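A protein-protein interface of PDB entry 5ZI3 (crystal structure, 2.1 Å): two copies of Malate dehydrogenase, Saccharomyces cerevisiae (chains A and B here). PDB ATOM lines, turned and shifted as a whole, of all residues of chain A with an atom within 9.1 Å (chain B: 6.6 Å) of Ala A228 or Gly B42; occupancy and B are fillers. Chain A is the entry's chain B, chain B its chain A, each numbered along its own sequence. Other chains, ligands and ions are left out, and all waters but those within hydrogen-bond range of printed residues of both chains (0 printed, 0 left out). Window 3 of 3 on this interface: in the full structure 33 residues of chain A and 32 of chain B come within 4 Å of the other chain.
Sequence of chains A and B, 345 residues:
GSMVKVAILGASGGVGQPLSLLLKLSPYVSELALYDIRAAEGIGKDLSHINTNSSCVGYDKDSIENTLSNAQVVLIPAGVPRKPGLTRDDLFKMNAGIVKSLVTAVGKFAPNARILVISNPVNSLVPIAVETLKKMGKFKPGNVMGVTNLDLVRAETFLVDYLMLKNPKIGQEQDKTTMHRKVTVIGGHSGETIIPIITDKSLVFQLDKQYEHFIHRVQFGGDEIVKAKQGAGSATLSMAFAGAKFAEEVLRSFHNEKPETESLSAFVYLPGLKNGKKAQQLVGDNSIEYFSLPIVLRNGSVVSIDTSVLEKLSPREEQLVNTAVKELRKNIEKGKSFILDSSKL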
ATOM      1  N   PHE A 220     -23.727  36.271 -21.031  1.00  0.00           N
ATOM      2  CA  PHE A 220     -23.022  35.039 -20.644  1.00  0.00           C
ATOM      3  C   PHE A 220     -23.627  34.292 -19.409  1.00  0.00           C
ATOM      4  O   PHE A 220     -23.023  33.388 -18.835  1.00  0.00           O
ATOM      5  CB  PHE A 220     -21.493  35.320 -20.637  1.00  0.00           C
ATOM      6  CG  PHE A 220     -20.942  35.571 -22.057  1.00  0.00           C
ATOM      7  CD1 PHE A 220     -20.770  34.509 -22.946  1.00  0.00           C
ATOM      8  CD2 PHE A 220     -20.707  36.847 -22.536  1.00  0.00           C
ATOM      9  CE1 PHE A 220     -20.339  34.715 -24.257  1.00  0.00           C
ATOM     10  CE2 PHE A 220     -20.268  37.079 -23.844  1.00  0.00           C
ATOM     11  CZ  PHE A 220     -20.056  36.013 -24.693  1.00  0.00           C
ATOM     12  N   GLY A 221     -24.870  34.638 -19.082  1.00  0.00           N
ATOM     13  CA  GLY A 221     -25.619  34.082 -17.943  1.00  0.00           C
ATOM     14  C   GLY A 221     -25.690  32.544 -17.962  1.00  0.00           C
ATOM     15  O   GLY A 221     -25.504  31.953 -16.957  1.00  0.00           O
ATOM     16  N   GLY A 222     -25.946  31.938 -19.114  1.00  0.00           N
ATOM     17  CA  GLY A 222     -25.922  30.471 -19.318  1.00  0.00           C
ATOM     18  C   GLY A 222     -24.622  29.824 -18.862  1.00  0.00           C
ATOM     19  O   GLY A 222     -24.670  28.826 -18.170  1.00  0.00           O
ATOM     20  N   ASP A 223     -23.484  30.416 -19.269  1.00  0.00           N
ATOM     21  CA  ASP A 223     -22.149  29.943 -18.975  1.00  0.00           C
ATOM     22  C   ASP A 223     -21.840  30.117 -17.520  1.00  0.00           C
ATOM     23  O   ASP A 223     -21.128  29.284 -16.922  1.00  0.00           O
ATOM     24  CB  ASP A 223     -21.061  30.719 -19.774  1.00  0.00           C
ATOM     25  CG  ASP A 223     -20.984  30.292 -21.218  1.00  0.00           C
ATOM     26  OD1 ASP A 223     -21.740  29.369 -21.613  1.00  0.00           O
ATOM     27  OD2 ASP A 223     -20.164  30.879 -21.974  1.00  0.00           O
ATOM     28  N   GLU A 224     -22.377  31.174 -16.917  1.00  0.00           N
ATOM     29  CA  GLU A 224     -22.158  31.384 -15.485  1.00  0.00           C
ATOM     30  C   GLU A 224     -22.750  30.237 -14.677  1.00  0.00           C
ATOM     31  O   GLU A 224     -22.196  29.830 -13.689  1.00  0.00           O
ATOM     32  CB  GLU A 224     -22.811  32.717 -15.062  1.00  0.00           C
ATOM     33  CG  GLU A 224     -22.814  33.077 -13.553  1.00  0.00           C
ATOM     34  CD  GLU A 224     -23.646  34.376 -13.253  1.00  0.00           C
ATOM     35  OE1 GLU A 224     -23.744  35.258 -14.123  1.00  0.00           O
ATOM     36  OE2 GLU A 224     -24.228  34.523 -12.170  1.00  0.00           O
ATOM     37  N   ILE A 225     -23.943  29.787 -15.019  1.00  0.00           N
ATOM     38  CA  ILE A 225     -24.549  28.693 -14.191  1.00  0.00           C
ATOM     39  C   ILE A 225     -23.803  27.374 -14.446  1.00  0.00           C
ATOM     40  O   ILE A 225     -23.600  26.634 -13.533  1.00  0.00           O
ATOM     41  CB  ILE A 225     -26.058  28.531 -14.433  1.00  0.00           C
ATOM     42  CG1 ILE A 225     -26.822  29.841 -14.175  1.00  0.00           C
ATOM     43  CG2 ILE A 225     -26.690  27.486 -13.517  1.00  0.00           C
ATOM     44  CD1 ILE A 225     -26.569  30.502 -12.833  1.00  0.00           C
ATOM     45  N   VAL A 226     -23.408  27.103 -15.689  1.00  0.00           N
ATOM     46  CA  VAL A 226     -22.697  25.859 -16.032  1.00  0.00           C
ATOM     47  C   VAL A 226     -21.460  25.882 -15.170  1.00  0.00           C
ATOM     48  O   VAL A 226     -21.222  24.956 -14.386  1.00  0.00           O
ATOM     49  CB  VAL A 226     -22.418  25.752 -17.540  1.00  0.00           C
ATOM     50  CG1 VAL A 226     -21.391  24.672 -17.913  1.00  0.00           C
ATOM     51  CG2 VAL A 226     -23.706  25.514 -18.273  1.00  0.00           C
ATOM     52  N   LYS A 227     -20.715  26.972 -15.217  1.00  0.00           N
ATOM     53  CA  LYS A 227     -19.550  27.107 -14.343  1.00  0.00           C
ATOM     54  C   LYS A 227     -19.905  26.910 -12.866  1.00  0.00           C
ATOM     55  O   LYS A 227     -19.176  26.239 -12.140  1.00  0.00           O
ATOM     56  CB  LYS A 227     -18.813  28.456 -14.581  1.00  0.00           C
ATOM     57  CG  LYS A 227     -17.792  28.809 -13.512  1.00  0.00           C
ATOM     58  CD  LYS A 227     -16.682  29.699 -14.060  1.00  0.00           C
ATOM     59  CE  LYS A 227     -15.528  29.738 -13.055  1.00  0.00           C
ATOM     60  NZ  LYS A 227     -14.309  30.377 -13.617  1.00  0.00           N
ATOM     61  N   ALA A 228     -21.021  27.446 -12.406  1.00  0.00           N
ATOM     62  CA  ALA A 228     -21.331  27.342 -10.999  1.00  0.00           C
ATOM     63  C   ALA A 228     -21.782  25.931 -10.607  1.00  0.00           C
ATOM     64  O   ALA A 228     -21.807  25.618  -9.439  1.00  0.00           O
ATOM     65  CB  ALA A 228     -22.371  28.365 -10.600  1.00  0.00           C
ATOM     66  N   LYS A 229     -22.174  25.101 -11.577  1.00  0.00           N
ATOM     67  CA  LYS A 229     -22.515  23.688 -11.319  1.00  0.00           C
ATOM     68  C   LYS A 229     -21.384  22.770 -11.832  1.00  0.00           C
ATOM     69  O   LYS A 229     -21.646  21.647 -12.213  1.00  0.00           O
ATOM     70  CB  LYS A 229     -23.825  23.316 -12.051  1.00  0.00           C
ATOM     71  CG  LYS A 229     -25.054  24.019 -11.540  1.00  0.00           C
ATOM     72  CD  LYS A 229     -26.306  23.663 -12.307  1.00  0.00           C
ATOM     73  CE  LYS A 229     -27.516  24.229 -11.567  1.00  0.00           C
ATOM     74  NZ  LYS A 229     -28.677  24.282 -12.495  1.00  0.00           N
ATOM     75  N   GLN A 230     -20.151  23.286 -11.865  1.00  0.00           N
ATOM     76  CA  GLN A 230     -18.975  22.691 -12.559  1.00  0.00           C
ATOM     77  C   GLN A 230     -19.250  21.825 -13.772  1.00  0.00           C
ATOM     78  O   GLN A 230     -19.027  20.618 -13.740  1.00  0.00           O
ATOM     79  CB  GLN A 230     -18.062  21.893 -11.616  1.00  0.00           C
ATOM     80  CG  GLN A 230     -17.533  22.645 -10.433  1.00  0.00           C
ATOM     81  CD  GLN A 230     -18.215  22.187  -9.175  1.00  0.00           C
ATOM     82  OE1 GLN A 230     -19.422  22.346  -9.043  1.00  0.00           O
ATOM     83  NE2 GLN A 230     -17.455  21.586  -8.251  1.00  0.00           N
ATOM     84  N   GLY A 231     -19.698  22.441 -14.851  1.00  0.00           N
ATOM     85  CA  GLY A 231     -20.000  21.728 -16.066  1.00  0.00           C
ATOM     86  C   GLY A 231     -21.230  20.823 -15.998  1.00  0.00           C
ATOM     87  O   GLY A 231     -21.732  20.396 -17.046  1.00  0.00           O
ATOM     88  N   ALA A 232     -21.740  20.523 -14.803  1.00  0.00           N
ATOM     89  CA  ALA A 232     -22.583  19.321 -14.661  1.00  0.00           C
ATOM     90  C   ALA A 232     -24.054  19.644 -14.652  1.00  0.00           C
ATOM     91  O   ALA A 232     -24.837  18.961 -14.029  1.00  0.00           O
ATOM     92  CB  ALA A 232     -22.203  18.539 -13.410  1.00  0.00           C
ATOM     93  N   GLY A 233     -24.412  20.679 -15.390  1.00  0.00           N
ATOM     94  CA  GLY A 233     -25.741  21.248 -15.379  1.00  0.00           C
ATOM     95  C   GLY A 233     -25.713  22.692 -15.886  1.00  0.00           C
ATOM     96  O   GLY A 233     -24.723  23.355 -15.865  1.00  0.00           O
ATOM     97  N   SER A 234     -26.845  23.162 -16.322  1.00  0.00           N
ATOM     98  CA  SER A 234     -27.016  24.513 -16.782  1.00  0.00           C
ATOM     99  C   SER A 234     -28.233  25.002 -16.016  1.00  0.00           C
ATOM    100  O   SER A 234     -28.669  24.355 -15.066  1.00  0.00           O
ATOM    101  CB  SER A 234     -27.273  24.424 -18.245  1.00  0.00           C
ATOM    102  OG  SER A 234     -27.972  23.207 -18.453  1.00  0.00           O
ATOM    103  N   ALA A 235     -28.801  26.119 -16.414  1.00  0.00           N
ATOM    104  CA  ALA A 235     -29.856  26.738 -15.669  1.00  0.00           C
ATOM    105  C   ALA A 235     -31.251  26.118 -15.844  1.00  0.00           C
ATOM    106  O   ALA A 235     -32.031  26.670 -16.583  1.00  0.00           O
ATOM    107  CB  ALA A 235     -29.907  28.206 -16.113  1.00  0.00           C
ATOM    108  N   THR A 236     -31.639  25.135 -15.044  1.00  0.00           N
ATOM    109  CA  THR A 236     -32.853  24.408 -15.256  1.00  0.00           C
ATOM    110  C   THR A 236     -34.079  25.122 -14.640  1.00  0.00           C
ATOM    111  O   THR A 236     -35.094  25.224 -15.265  1.00  0.00           O
ATOM    112  CB  THR A 236     -32.724  23.005 -14.658  1.00  0.00           C
ATOM    113  OG1 THR A 236     -32.158  23.151 -13.371  1.00  0.00           O
ATOM    114  CG2 THR A 236     -31.784  22.137 -15.458  1.00  0.00           C
ATOM    115  N   LEU A 237     -33.985  25.553 -13.411  1.00  0.00           N
ATOM    116  CA  LEU A 237     -35.124  26.086 -12.698  1.00  0.00           C
ATOM    117  C   LEU A 237     -35.500  27.493 -13.248  1.00  0.00           C
ATOM    118  O   LEU A 237     -36.697  27.807 -13.476  1.00  0.00           O
ATOM    119  CB  LEU A 237     -34.801  26.176 -11.234  1.00  0.00           C
ATOM    120  CG  LEU A 237     -34.381  24.868 -10.584  1.00  0.00           C
ATOM    121  CD1 LEU A 237     -33.870  25.180  -9.212  1.00  0.00           C
ATOM    122  CD2 LEU A 237     -35.561  23.889 -10.527  1.00  0.00           C
ATOM    123  N   SER A 238     -34.488  28.306 -13.535  1.00  0.00           N
ATOM    124  CA  SER A 238     -34.776  29.579 -14.151  1.00  0.00           C
ATOM    125  C   SER A 238     -35.236  29.444 -15.587  1.00  0.00           C
ATOM    126  O   SER A 238     -36.012  30.263 -15.979  1.00  0.00           O
ATOM    127  CB  SER A 238     -33.605  30.538 -14.036  1.00  0.00           C
ATOM    128  OG  SER A 238     -32.512  29.994 -14.643  1.00  0.00           O
ATOM    129  N   ALA B  39     -24.532  20.532  -4.173  1.00  0.00           N
ATOM    130  CA  ALA B  39     -25.245  21.184  -5.276  1.00  0.00           C
ATOM    131  C   ALA B  39     -26.030  22.443  -4.951  1.00  0.00           C
ATOM    132  O   ALA B  39     -26.544  23.066  -5.894  1.00  0.00           O
ATOM    133  CB  ALA B  39     -26.143  20.180  -6.005  1.00  0.00           C
ATOM    134  N   ALA B  40     -26.092  22.849  -3.684  1.00  0.00           N
ATOM    135  CA  ALA B  40     -26.923  24.002  -3.322  1.00  0.00           C
ATOM    136  C   ALA B  40     -26.397  25.332  -3.863  1.00  0.00           C
ATOM    137  O   ALA B  40     -27.187  26.214  -4.209  1.00  0.00           O
ATOM    138  CB  ALA B  40     -27.126  24.123  -1.831  1.00  0.00           C
ATOM    139  N   GLU B  41     -25.088  25.469  -3.928  1.00  0.00           N
ATOM    140  CA  GLU B  41     -24.484  26.684  -4.549  1.00  0.00           C
ATOM    141  C   GLU B  41     -24.979  26.935  -5.948  1.00  0.00           C
ATOM    142  O   GLU B  41     -25.428  28.037  -6.261  1.00  0.00           O
ATOM    143  CB  GLU B  41     -22.975  26.615  -4.510  1.00  0.00           C
ATOM    144  CG  GLU B  41     -22.454  26.653  -3.064  1.00  0.00           C
ATOM    145  CD  GLU B  41     -21.076  25.979  -2.922  1.00  0.00           C
ATOM    146  OE1 GLU B  41     -20.966  24.728  -2.998  1.00  0.00           O
ATOM    147  OE2 GLU B  41     -20.103  26.699  -2.697  1.00  0.00           O
ATOM    148  N   GLY B  42     -24.917  25.909  -6.782  1.00  0.00           N
ATOM    149  CA  GLY B  42     -25.339  26.008  -8.136  1.00  0.00           C
ATOM    150  C   GLY B  42     -26.823  26.295  -8.302  1.00  0.00           C
ATOM    151  O   GLY B  42     -27.208  27.097  -9.144  1.00  0.00           O
ATOM    152  N   ILE B  43     -27.626  25.618  -7.506  1.00  0.00           N
ATOM    153  CA  ILE B  43     -29.053  25.780  -7.528  1.00  0.00           C
ATOM    154  C   ILE B  43     -29.377  27.150  -7.061  1.00  0.00           C
ATOM    155  O   ILE B  43     -30.199  27.823  -7.688  1.00  0.00           O
ATOM    156  CB  ILE B  43     -29.788  24.780  -6.641  1.00  0.00           C
ATOM    157  CG1 ILE B  43     -29.609  23.405  -7.226  1.00  0.00           C
ATOM    158  CG2 ILE B  43     -31.275  25.133  -6.557  1.00  0.00           C
ATOM    159  CD1 ILE B  43     -29.915  22.308  -6.227  1.00  0.00           C
ATOM    160  N   GLY B  44     -28.730  27.586  -6.000  1.00  0.00           N
ATOM    161  CA  GLY B  44     -28.897  28.985  -5.548  1.00  0.00           C
ATOM    162  C   GLY B  44     -28.539  30.007  -6.628  1.00  0.00           C
ATOM    163  O   GLY B  44     -29.235  31.001  -6.805  1.00  0.00           O
ATOM    164  N   LYS B  45     -27.455  29.760  -7.368  1.00  0.00           N
ATOM    165  CA  LYS B  45     -27.013  30.683  -8.406  1.00  0.00           C
ATOM    166  C   LYS B  45     -28.035  30.706  -9.558  1.00  0.00           C
ATOM    167  O   LYS B  45     -28.332  31.750 -10.071  1.00  0.00           O
ATOM    168  CB  LYS B  45     -25.616  30.338  -8.937  1.00  0.00           C
ATOM    169  CG  LYS B  45     -24.455  30.955  -8.176  1.00  0.00           C
ATOM    170  CD  LYS B  45     -24.388  32.481  -8.211  1.00  0.00           C
ATOM    171  CE  LYS B  45     -23.258  32.967  -9.114  1.00  0.00           C
ATOM    172  NZ  LYS B  45     -23.236  34.455  -9.193  1.00  0.00           N
ATOM    173  N   ASP B  46     -28.546  29.534  -9.955  1.00  0.00           N
ATOM    174  CA  ASP B  46     -29.605  29.414 -10.980  1.00  0.00           C
ATOM    175  C   ASP B  46     -30.820  30.309 -10.613  1.00  0.00           C
ATOM    176  O   ASP B  46     -31.267  31.223 -11.376  1.00  0.00           O
ATOM    177  CB  ASP B  46     -29.966  27.887 -11.113  1.00  0.00           C
ATOM    178  CG  ASP B  46     -31.069  27.587 -12.147  1.00  0.00           C
ATOM    179  OD1 ASP B  46     -31.708  28.488 -12.717  1.00  0.00           O
ATOM    180  OD2 ASP B  46     -31.224  26.417 -12.471  1.00  0.00           O
ATOM    181  N   LEU B  47     -31.315  30.083  -9.404  1.00  0.00           N
ATOM    182  CA  LEU B  47     -32.480  30.772  -8.916  1.00  0.00           C
ATOM    183  C   LEU B  47     -32.221  32.264  -8.724  1.00  0.00           C
ATOM    184  O   LEU B  47     -33.127  33.041  -8.906  1.00  0.00           O
ATOM    185  CB  LEU B  47     -32.964  30.168  -7.615  1.00  0.00           C
ATOM    186  CG  LEU B  47     -33.600  28.797  -7.687  1.00  0.00           C
ATOM    187  CD1 LEU B  47     -33.861  28.265  -6.294  1.00  0.00           C
ATOM    188  CD2 LEU B  47     -34.874  28.767  -8.528  1.00  0.00           C
ATOM    189  N   GLY B  58     -26.993  30.027  -2.229  1.00  0.00           N
ATOM    190  CA  GLY B  58     -26.865  28.634  -1.816  1.00  0.00           C
ATOM    191  C   GLY B  58     -25.544  28.392  -1.105  1.00  0.00           C
ATOM    192  O   GLY B  58     -24.585  29.081  -1.353  1.00  0.00           O
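The side-chain amino group (NZ) of Lys A229 sits at hydrogen-bond distance from the backbone carbonyl oxygen (O) of Ser A234 (2.6 Å).
The side-chain hydroxyl (OG) of Ser A238 sits at hydrogen-bond distance from the side-chain carboxylate (OD1) of Asp B46 (2.6 Å).
The side-chain carboxylate of Asp B46 is in hydrogen-bond range of the backbone NH of Leu A237.
NZ of Lys B45 is in salt-bridge range of OE2 of Glu A224 (3.1 Å).
OD2 of Asp B46 sits at hydrogen-bond distance from N of Thr A236 (2.9 Å).
The side-chain carboxylate (OD2) of Asp B46 is in salt-bridge range of the side-chain amino group (NZ) of Lys A229 (3.3 Å).
Lys B45 touches Ile A225 (O to CD1, 3.5 Å).
Asp B46 touches Ile A225 (N to CD1, 3.6 Å).
Ala A228 touches Gly B42 (O to CA, 3.8 Å).
CE of Lys A229 touches O of Gly B42, 3.8 Å away.
Ala A235 touches Asp B46 (C to OD2, 3.4 Å).
Leu A237 touches Ile B43.
Leu A237 touches Leu B47.
Of chain B, only Gly B42 (3.8 Å) comes within 4 Å of Ala A228.
Gly B42 touches two residues of chain A.
No residue of chain A comes within 4 Å of Gly B44.
Of the printed residues of chain B, Ile A225 touches Lys B45 and Asp B46.
Of the printed residues of chain B, Glu A224 touches Lys B45.
Of the printed residues of chain A, Leu B47 touches Leu A237 (3.7 Å).
Of the printed residues of chain B, Lys A229 touches Gly B42 and Asp B46.
Printed residues of chain B within 4 Å of Thr A236: Asp B46.
Gly A222 touches none of the printed residues of chain B.
The nearest residue of chain B that does not touch Ala A228 is Lys B45 (4.1 Å).
The nearest residue of chain A that does not touch Gly B42 is Ile A225 (4.4 Å).
The nearest printed residue of chain B that does not touch Ser A238 is Leu B47 (5.0 Å).
Of the 10 printed residues of chain B, 5 touch a printed residue of chain A.
Hydrophobic or aromatic side chains of chain B that line the printed part of chain A: Ile B43 and Leu B47.
Printed residues of chain A that touch a printed residue of chain B: Glu A224, Ile A225, Ala A228, Lys A229, Ala A235, Thr A236, Leu A237 and Ser A238.
Among the printed residues, 12 pairs touch across the chains.
Among the printed residues, Asp or Glu carboxylates within 4 Å of a Lys or Arg side-chain nitrogen of the other chain: Glu A224 with Lys B45 and Lys A229 with Asp B46.
No position is printed for both chains.
Of the 12 pairs that touch across the chains among the printed residues, none has its exchanged pair printed and touching as well.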
